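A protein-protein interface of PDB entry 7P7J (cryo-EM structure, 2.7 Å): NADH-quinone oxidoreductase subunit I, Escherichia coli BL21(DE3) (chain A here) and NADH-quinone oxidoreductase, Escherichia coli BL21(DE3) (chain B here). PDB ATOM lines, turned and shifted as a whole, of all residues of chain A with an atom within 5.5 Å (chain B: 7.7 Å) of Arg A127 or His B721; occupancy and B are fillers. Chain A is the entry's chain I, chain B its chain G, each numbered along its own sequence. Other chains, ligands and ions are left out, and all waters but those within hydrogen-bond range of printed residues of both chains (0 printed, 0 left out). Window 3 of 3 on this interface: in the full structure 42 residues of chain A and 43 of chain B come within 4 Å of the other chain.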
ATOM      1  N   ASN A  95      16.986   5.644  -3.203  1.00  0.00           N
ATOM      2  CA  ASN A  95      17.616   5.530  -1.895  1.00  0.00           C
ATOM      3  C   ASN A  95      18.248   6.877  -1.579  1.00  0.00           C
ATOM      4  O   ASN A  95      19.366   7.164  -2.004  1.00  0.00           O
ATOM      5  CB  ASN A  95      18.640   4.402  -1.894  1.00  0.00           C
ATOM      6  CG  ASN A  95      19.262   4.178  -0.535  1.00  0.00           C
ATOM      7  OD1 ASN A  95      18.735   4.612   0.484  1.00  0.00           O
ATOM      8  ND2 ASN A  95      20.384   3.483  -0.515  1.00  0.00           N
ATOM      9  N   SER A  97      19.417   7.962   1.156  1.00  0.00           N
ATOM     10  CA  SER A  97      20.617   7.887   1.975  1.00  0.00           C
ATOM     11  C   SER A  97      21.877   7.814   1.126  1.00  0.00           C
ATOM     12  O   SER A  97      22.966   8.104   1.627  1.00  0.00           O
ATOM     13  CB  SER A  97      20.546   6.683   2.909  1.00  0.00           C
ATOM     14  OG  SER A  97      20.795   5.481   2.210  1.00  0.00           O
ATOM     15  N   ARG A  98      21.754   7.429  -0.141  1.00  0.00           N
ATOM     16  CA  ARG A  98      22.879   7.376  -1.062  1.00  0.00           C
ATOM     17  C   ARG A  98      22.937   8.568  -1.999  1.00  0.00           C
ATOM     18  O   ARG A  98      24.026   8.919  -2.457  1.00  0.00           O
ATOM     19  CB  ARG A  98      22.818   6.100  -1.905  1.00  0.00           C
ATOM     20  CG  ARG A  98      23.355   4.865  -1.228  1.00  0.00           C
ATOM     21  CD  ARG A  98      24.844   4.723  -1.395  1.00  0.00           C
ATOM     22  NE  ARG A  98      25.307   3.454  -0.852  1.00  0.00           N
ATOM     23  CZ  ARG A  98      26.573   3.064  -0.830  1.00  0.00           C
ATOM     24  NH1 ARG A  98      27.538   3.828  -1.309  1.00  0.00           N
ATOM     25  NH2 ARG A  98      26.877   1.878  -0.314  1.00  0.00           N
ATOM     26  N   TYR A 125      14.670   9.593  11.020  1.00  0.00           N
ATOM     27  CA  TYR A 125      15.142   8.884  12.204  1.00  0.00           C
ATOM     28  C   TYR A 125      15.746   7.531  11.849  1.00  0.00           C
ATOM     29  O   TYR A 125      16.715   7.099  12.480  1.00  0.00           O
ATOM     30  CB  TYR A 125      14.000   8.707  13.203  1.00  0.00           C
ATOM     31  CG  TYR A 125      13.415  10.006  13.694  1.00  0.00           C
ATOM     32  CD1 TYR A 125      14.112  10.808  14.583  1.00  0.00           C
ATOM     33  CD2 TYR A 125      12.166  10.429  13.271  1.00  0.00           C
ATOM     34  CE1 TYR A 125      13.586  11.997  15.032  1.00  0.00           C
ATOM     35  CE2 TYR A 125      11.631  11.616  13.718  1.00  0.00           C
ATOM     36  CZ  TYR A 125      12.345  12.394  14.599  1.00  0.00           C
ATOM     37  OH  TYR A 125      11.821  13.578  15.050  1.00  0.00           O
ATOM     38  N   LYS A 126      15.191   6.851  10.851  1.00  0.00           N
ATOM     39  CA  LYS A 126      15.681   5.557  10.405  1.00  0.00           C
ATOM     40  C   LYS A 126      16.199   5.679   8.982  1.00  0.00           C
ATOM     41  O   LYS A 126      15.616   6.391   8.161  1.00  0.00           O
ATOM     42  CB  LYS A 126      14.587   4.493  10.469  1.00  0.00           C
ATOM     43  CG  LYS A 126      13.870   4.419  11.800  1.00  0.00           C
ATOM     44  CD  LYS A 126      14.551   3.443  12.738  1.00  0.00           C
ATOM     45  CE  LYS A 126      14.273   3.793  14.186  1.00  0.00           C
ATOM     46  NZ  LYS A 126      15.526   3.916  14.979  1.00  0.00           N
ATOM     47  N   ARG A 127      17.307   4.992   8.699  1.00  0.00           N
ATOM     48  CA  ARG A 127      17.879   5.035   7.359  1.00  0.00           C
ATOM     49  C   ARG A 127      17.021   4.272   6.358  1.00  0.00           C
ATOM     50  O   ARG A 127      17.037   4.592   5.164  1.00  0.00           O
ATOM     51  CB  ARG A 127      19.300   4.476   7.384  1.00  0.00           C
ATOM     52  CG  ARG A 127      20.123   4.792   6.154  1.00  0.00           C
ATOM     53  CD  ARG A 127      21.506   4.194   6.264  1.00  0.00           C
ATOM     54  NE  ARG A 127      21.883   3.485   5.051  1.00  0.00           N
ATOM     55  CZ  ARG A 127      22.907   2.651   4.956  1.00  0.00           C
ATOM     56  NH1 ARG A 127      23.686   2.394   5.991  1.00  0.00           N
ATOM     57  NH2 ARG A 127      23.152   2.056   3.795  1.00  0.00           N
ATOM     58  N   GLN A 128      16.273   3.267   6.820  1.00  0.00           N
ATOM     59  CA  GLN A 128      15.370   2.535   5.938  1.00  0.00           C
ATOM     60  C   GLN A 128      14.250   3.425   5.419  1.00  0.00           C
ATOM     61  O   GLN A 128      13.730   3.196   4.323  1.00  0.00           O
ATOM     62  CB  GLN A 128      14.791   1.328   6.674  1.00  0.00           C
ATOM     63  CG  GLN A 128      14.078   0.334   5.787  1.00  0.00           C
ATOM     64  CD  GLN A 128      14.986  -0.247   4.731  1.00  0.00           C
ATOM     65  OE1 GLN A 128      16.100  -0.677   5.025  1.00  0.00           O
ATOM     66  NE2 GLN A 128      14.521  -0.258   3.491  1.00  0.00           N
ATOM     67  N   ASP A 129      13.888   4.455   6.175  1.00  0.00           N
ATOM     68  CA  ASP A 129      12.841   5.378   5.774  1.00  0.00           C
ATOM     69  C   ASP A 129      13.316   6.407   4.759  1.00  0.00           C
ATOM     70  O   ASP A 129      12.500   7.193   4.271  1.00  0.00           O
ATOM     71  CB  ASP A 129      12.288   6.077   7.011  1.00  0.00           C
ATOM     72  CG  ASP A 129      11.492   5.141   7.891  1.00  0.00           C
ATOM     73  OD1 ASP A 129      10.872   4.202   7.352  1.00  0.00           O
ATOM     74  OD2 ASP A 129      11.500   5.331   9.124  1.00  0.00           O
ATOM     75  N   LEU A 130      14.604   6.428   4.437  1.00  0.00           N
ATOM     76  CA  LEU A 130      15.130   7.272   3.377  1.00  0.00           C
ATOM     77  C   LEU A 130      15.039   6.614   2.010  1.00  0.00           C
ATOM     78  O   LEU A 130      15.428   7.229   1.014  1.00  0.00           O
ATOM     79  CB  LEU A 130      16.580   7.650   3.669  1.00  0.00           C
ATOM     80  CG  LEU A 130      16.788   8.757   4.698  1.00  0.00           C
ATOM     81  CD1 LEU A 130      18.255   8.866   5.078  1.00  0.00           C
ATOM     82  CD2 LEU A 130      16.266  10.072   4.164  1.00  0.00           C
ATOM     83  N   VAL A 131      14.550   5.382   1.940  1.00  0.00           N
ATOM     84  CA  VAL A 131      14.251   4.730   0.671  1.00  0.00           C
ATOM     85  C   VAL A 131      12.834   5.134   0.287  1.00  0.00           C
ATOM     86  O   VAL A 131      11.861   4.668   0.883  1.00  0.00           O
ATOM     87  CB  VAL A 131      14.399   3.208   0.766  1.00  0.00           C
ATOM     88  CG1 VAL A 131      13.968   2.553  -0.527  1.00  0.00           C
ATOM     89  CG2 VAL A 131      15.829   2.842   1.092  1.00  0.00           C
ATOM     90  N   ARG B 711      22.793  -0.290  -8.185  1.00  0.00           N
ATOM     91  CA  ARG B 711      23.438  -1.234  -7.281  1.00  0.00           C
ATOM     92  C   ARG B 711      23.205  -0.915  -5.812  1.00  0.00           C
ATOM     93  O   ARG B 711      23.342  -1.808  -4.972  1.00  0.00           O
ATOM     94  CB  ARG B 711      24.936  -1.293  -7.562  1.00  0.00           C
ATOM     95  CG  ARG B 711      25.596   0.059  -7.703  1.00  0.00           C
ATOM     96  CD  ARG B 711      27.019  -0.114  -8.177  1.00  0.00           C
ATOM     97  NE  ARG B 711      27.696  -1.146  -7.404  1.00  0.00           N
ATOM     98  CZ  ARG B 711      28.448  -0.905  -6.340  1.00  0.00           C
ATOM     99  NH1 ARG B 711      28.669   0.329  -5.919  1.00  0.00           N
ATOM    100  NH2 ARG B 711      28.993  -1.926  -5.684  1.00  0.00           N
ATOM    101  N   THR B 712      22.857   0.324  -5.476  1.00  0.00           N
ATOM    102  CA  THR B 712      22.497   0.670  -4.110  1.00  0.00           C
ATOM    103  C   THR B 712      20.998   0.873  -3.937  1.00  0.00           C
ATOM    104  O   THR B 712      20.576   1.459  -2.938  1.00  0.00           O
ATOM    105  CB  THR B 712      23.255   1.918  -3.653  1.00  0.00           C
ATOM    106  OG1 THR B 712      22.882   3.034  -4.465  1.00  0.00           O
ATOM    107  CG2 THR B 712      24.746   1.696  -3.765  1.00  0.00           C
ATOM    108  N   ARG B 715      17.894  -3.694  -3.979  1.00  0.00           N
ATOM    109  CA  ARG B 715      17.519  -4.425  -2.781  1.00  0.00           C
ATOM    110  C   ARG B 715      17.218  -3.488  -1.618  1.00  0.00           C
ATOM    111  O   ARG B 715      17.153  -3.931  -0.470  1.00  0.00           O
ATOM    112  CB  ARG B 715      18.622  -5.412  -2.408  1.00  0.00           C
ATOM    113  CG  ARG B 715      18.113  -6.743  -1.914  1.00  0.00           C
ATOM    114  CD  ARG B 715      19.258  -7.626  -1.485  1.00  0.00           C
ATOM    115  NE  ARG B 715      18.823  -8.703  -0.607  1.00  0.00           N
ATOM    116  CZ  ARG B 715      18.830  -8.635   0.716  1.00  0.00           C
ATOM    117  NH1 ARG B 715      19.244  -7.551   1.349  1.00  0.00           N
ATOM    118  NH2 ARG B 715      18.411  -9.681   1.421  1.00  0.00           N
ATOM    119  N   ALA B 716      17.030  -2.198  -1.900  1.00  0.00           N
ATOM    120  CA  ALA B 716      16.799  -1.225  -0.842  1.00  0.00           C
ATOM    121  C   ALA B 716      15.416  -1.352  -0.224  1.00  0.00           C
ATOM    122  O   ALA B 716      15.212  -0.882   0.899  1.00  0.00           O
ATOM    123  CB  ALA B 716      17.006   0.192  -1.375  1.00  0.00           C
ATOM    124  N   ILE B 718      14.164  -4.243   0.588  1.00  0.00           N
ATOM    125  CA  ILE B 718      14.369  -5.262   1.612  1.00  0.00           C
ATOM    126  C   ILE B 718      15.168  -4.690   2.776  1.00  0.00           C
ATOM    127  O   ILE B 718      14.739  -4.742   3.934  1.00  0.00           O
ATOM    128  CB  ILE B 718      15.053  -6.502   1.009  1.00  0.00           C
ATOM    129  CG1 ILE B 718      14.073  -7.270   0.124  1.00  0.00           C
ATOM    130  CG2 ILE B 718      15.591  -7.410   2.100  1.00  0.00           C
ATOM    131  CD1 ILE B 718      14.357  -7.141  -1.345  1.00  0.00           C
ATOM    132  N   SER B 719      16.335  -4.124   2.483  1.00  0.00           N
ATOM    133  CA  SER B 719      17.135  -3.450   3.494  1.00  0.00           C
ATOM    134  C   SER B 719      17.976  -2.384   2.815  1.00  0.00           C
ATOM    135  O   SER B 719      18.495  -2.602   1.720  1.00  0.00           O
ATOM    136  CB  SER B 719      18.034  -4.428   4.255  1.00  0.00           C
ATOM    137  OG  SER B 719      19.049  -4.943   3.415  1.00  0.00           O
ATOM    138  N   VAL B 720      18.116  -1.234   3.481  1.00  0.00           N
ATOM    139  CA  VAL B 720      18.922  -0.150   2.938  1.00  0.00           C
ATOM    140  C   VAL B 720      20.404  -0.511   2.923  1.00  0.00           C
ATOM    141  O   VAL B 720      21.171   0.060   2.140  1.00  0.00           O
ATOM    142  CB  VAL B 720      18.643   1.150   3.726  1.00  0.00           C
ATOM    143  CG1 VAL B 720      19.278   1.113   5.106  1.00  0.00           C
ATOM    144  CG2 VAL B 720      19.102   2.375   2.945  1.00  0.00           C
ATOM    145  N   HIS B 721      20.826  -1.469   3.743  1.00  0.00           N
ATOM    146  CA  HIS B 721      22.212  -1.909   3.725  1.00  0.00           C
ATOM    147  C   HIS B 721      22.467  -2.778   2.503  1.00  0.00           C
ATOM    148  O   HIS B 721      21.728  -3.730   2.242  1.00  0.00           O
ATOM    149  CB  HIS B 721      22.538  -2.672   5.004  1.00  0.00           C
ATOM    150  CG  HIS B 721      22.322  -1.872   6.247  1.00  0.00           C
ATOM    151  ND1 HIS B 721      23.300  -1.073   6.796  1.00  0.00           N
ATOM    152  CD2 HIS B 721      21.234  -1.737   7.041  1.00  0.00           C
ATOM    153  CE1 HIS B 721      22.825  -0.481   7.877  1.00  0.00           C
ATOM    154  NE2 HIS B 721      21.574  -0.867   8.046  1.00  0.00           N
ATOM    155  N   GLU B 722      23.508  -2.439   1.753  1.00  0.00           N
ATOM    156  CA  GLU B 722      23.845  -3.198   0.558  1.00  0.00           C
ATOM    157  C   GLU B 722      24.324  -4.592   0.947  1.00  0.00           C
ATOM    158  O   GLU B 722      25.167  -4.724   1.841  1.00  0.00           O
ATOM    159  CB  GLU B 722      24.919  -2.479  -0.254  1.00  0.00           C
ATOM    160  CG  GLU B 722      24.373  -1.556  -1.322  1.00  0.00           C
ATOM    161  CD  GLU B 722      23.802  -0.278  -0.751  1.00  0.00           C
ATOM    162  OE1 GLU B 722      24.589   0.614  -0.381  1.00  0.00           O
ATOM    163  OE2 GLU B 722      22.562  -0.167  -0.669  1.00  0.00           O
ATOM    164  N   PRO B 723      23.812  -5.642   0.314  1.00  0.00           N
ATOM    165  CA  PRO B 723      24.250  -6.997   0.653  1.00  0.00           C
ATOM    166  C   PRO B 723      25.659  -7.257   0.149  1.00  0.00           C
ATOM    167  O   PRO B 723      26.217  -6.507  -0.654  1.00  0.00           O
ATOM    168  CB  PRO B 723      23.233  -7.880  -0.068  1.00  0.00           C
ATOM    169  CG  PRO B 723      22.839  -7.069  -1.244  1.00  0.00           C
ATOM    170  CD  PRO B 723      22.825  -5.643  -0.777  1.00  0.00           C
ATOM    171  N   ARG B 724      26.237  -8.342   0.649  1.00  0.00           N
ATOM    172  CA  ARG B 724      27.532  -8.781   0.158  1.00  0.00           C
ATOM    173  C   ARG B 724      27.411  -9.228  -1.291  1.00  0.00           C
ATOM    174  O   ARG B 724      26.407  -9.820  -1.693  1.00  0.00           O
ATOM    175  CB  ARG B 724      28.072  -9.919   1.023  1.00  0.00           C
ATOM    176  CG  ARG B 724      29.538 -10.225   0.779  1.00  0.00           C
ATOM    177  CD  ARG B 724      30.013 -11.451   1.574  1.00  0.00           C
ATOM    178  NE  ARG B 724      31.426 -11.515   1.969  1.00  0.00           N
ATOM    179  CZ  ARG B 724      32.501 -11.165   1.264  1.00  0.00           C
ATOM    180  NH1 ARG B 724      32.452 -10.936  -0.040  1.00  0.00           N
ATOM    181  NH2 ARG B 724      33.681 -11.117   1.875  1.00  0.00           N
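The side-chain amide oxygen (OE1) of Gln A128 lies within hydrogen-bond range of the backbone NH (N) of Val B720, 2.6 Å away.
The backbone carbonyl oxygen of Val B720 is in hydrogen-bond range of the guanidinium group of Arg A127 (3.3 Å).
O of Ala B716 is in hydrogen-bond range of NE2 of Gln A128, at 2.8 Å.
The side-chain carboxylate (OE1) of Glu B722 lies within salt-bridge range of the guanidinium group (NH2) of Arg A98, 2.6 Å away.
O of Thr B712 lies within hydrogen-bond range of ND2 of Asn A95, 3.2 Å away.
Among the printed residues, merely in contact across the chains: Asn A95 with Val B720 (3.3 Å), Ser A97 with Val B720 (3.6 Å), Arg A98 with Thr B712 (3.4 Å), Arg A127 with His B721 (3.5 Å), Gln A128 with Ser B719 (3.3 Å), Val A131 with Ala B716 (3.8 Å) and Val A131 with Val B720 (3.8 Å).
O of His B721 sits at hydrogen-bond distance from OG of Ser B719, 3.2 Å away.
The side-chain hydroxyl of Ser B719 sits at hydrogen-bond distance from the guanidinium group of Arg B715 (3.3 Å).
The side-chain amide oxygen (OD1) of Asn A95 is in hydrogen-bond range of the side-chain hydroxyl (OG) of Ser A97, 2.8 Å away.
Of the 10 printed residues of chain A, 6 touch a printed residue of chain B.
Printed residues of chain A that touch a printed residue of chain B: Asn A95, Ser A97, Arg A98, Arg A127, Gln A128 and Val A131.
Hydrophobic or aromatic side chains of chain A within 4 Å of the printed part of chain B: Val A131.
Of the 11 printed residues of chain B, 6 touch a printed residue of chain A.
Printed residues of chain B that touch a printed residue of chain A: Thr B712, Ala B716, Ser B719, Val B720, His B721 and Glu B722.
Hydrophobic or aromatic side chains of chain B within 4 Å of the printed part of chain A: Ala B716, Val B720 and His B721.
Among the printed residues, 12 pairs touch across the chains.
Printed residues of chain B within 4 Å of Asn A95: Thr B712 and Val B720.
Of chain B, only Val B720 and His B721 come within 4 Å of Arg A127.
Printed residues of chain B within 4 Å of Gln A128: Ala B716, Ser B719 and Val B720.
Arg B711 touches none of the printed residues of chain A.
Of the printed residues of chain A, Thr B712 touches Asn A95 and Arg A98.
Of the printed residues of chain A, Val B720 touches Asn A95, Ser A97, Arg A127, Gln A128 and Val A131.
Of chain A, only Arg A127 (3.5 Å) comes within 4 Å of His B721.
Printed residues of chain A within 4 Å of Glu B722: Arg A98 (2.6 Å).
Pro B723 touches none of the printed residues of chain A.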
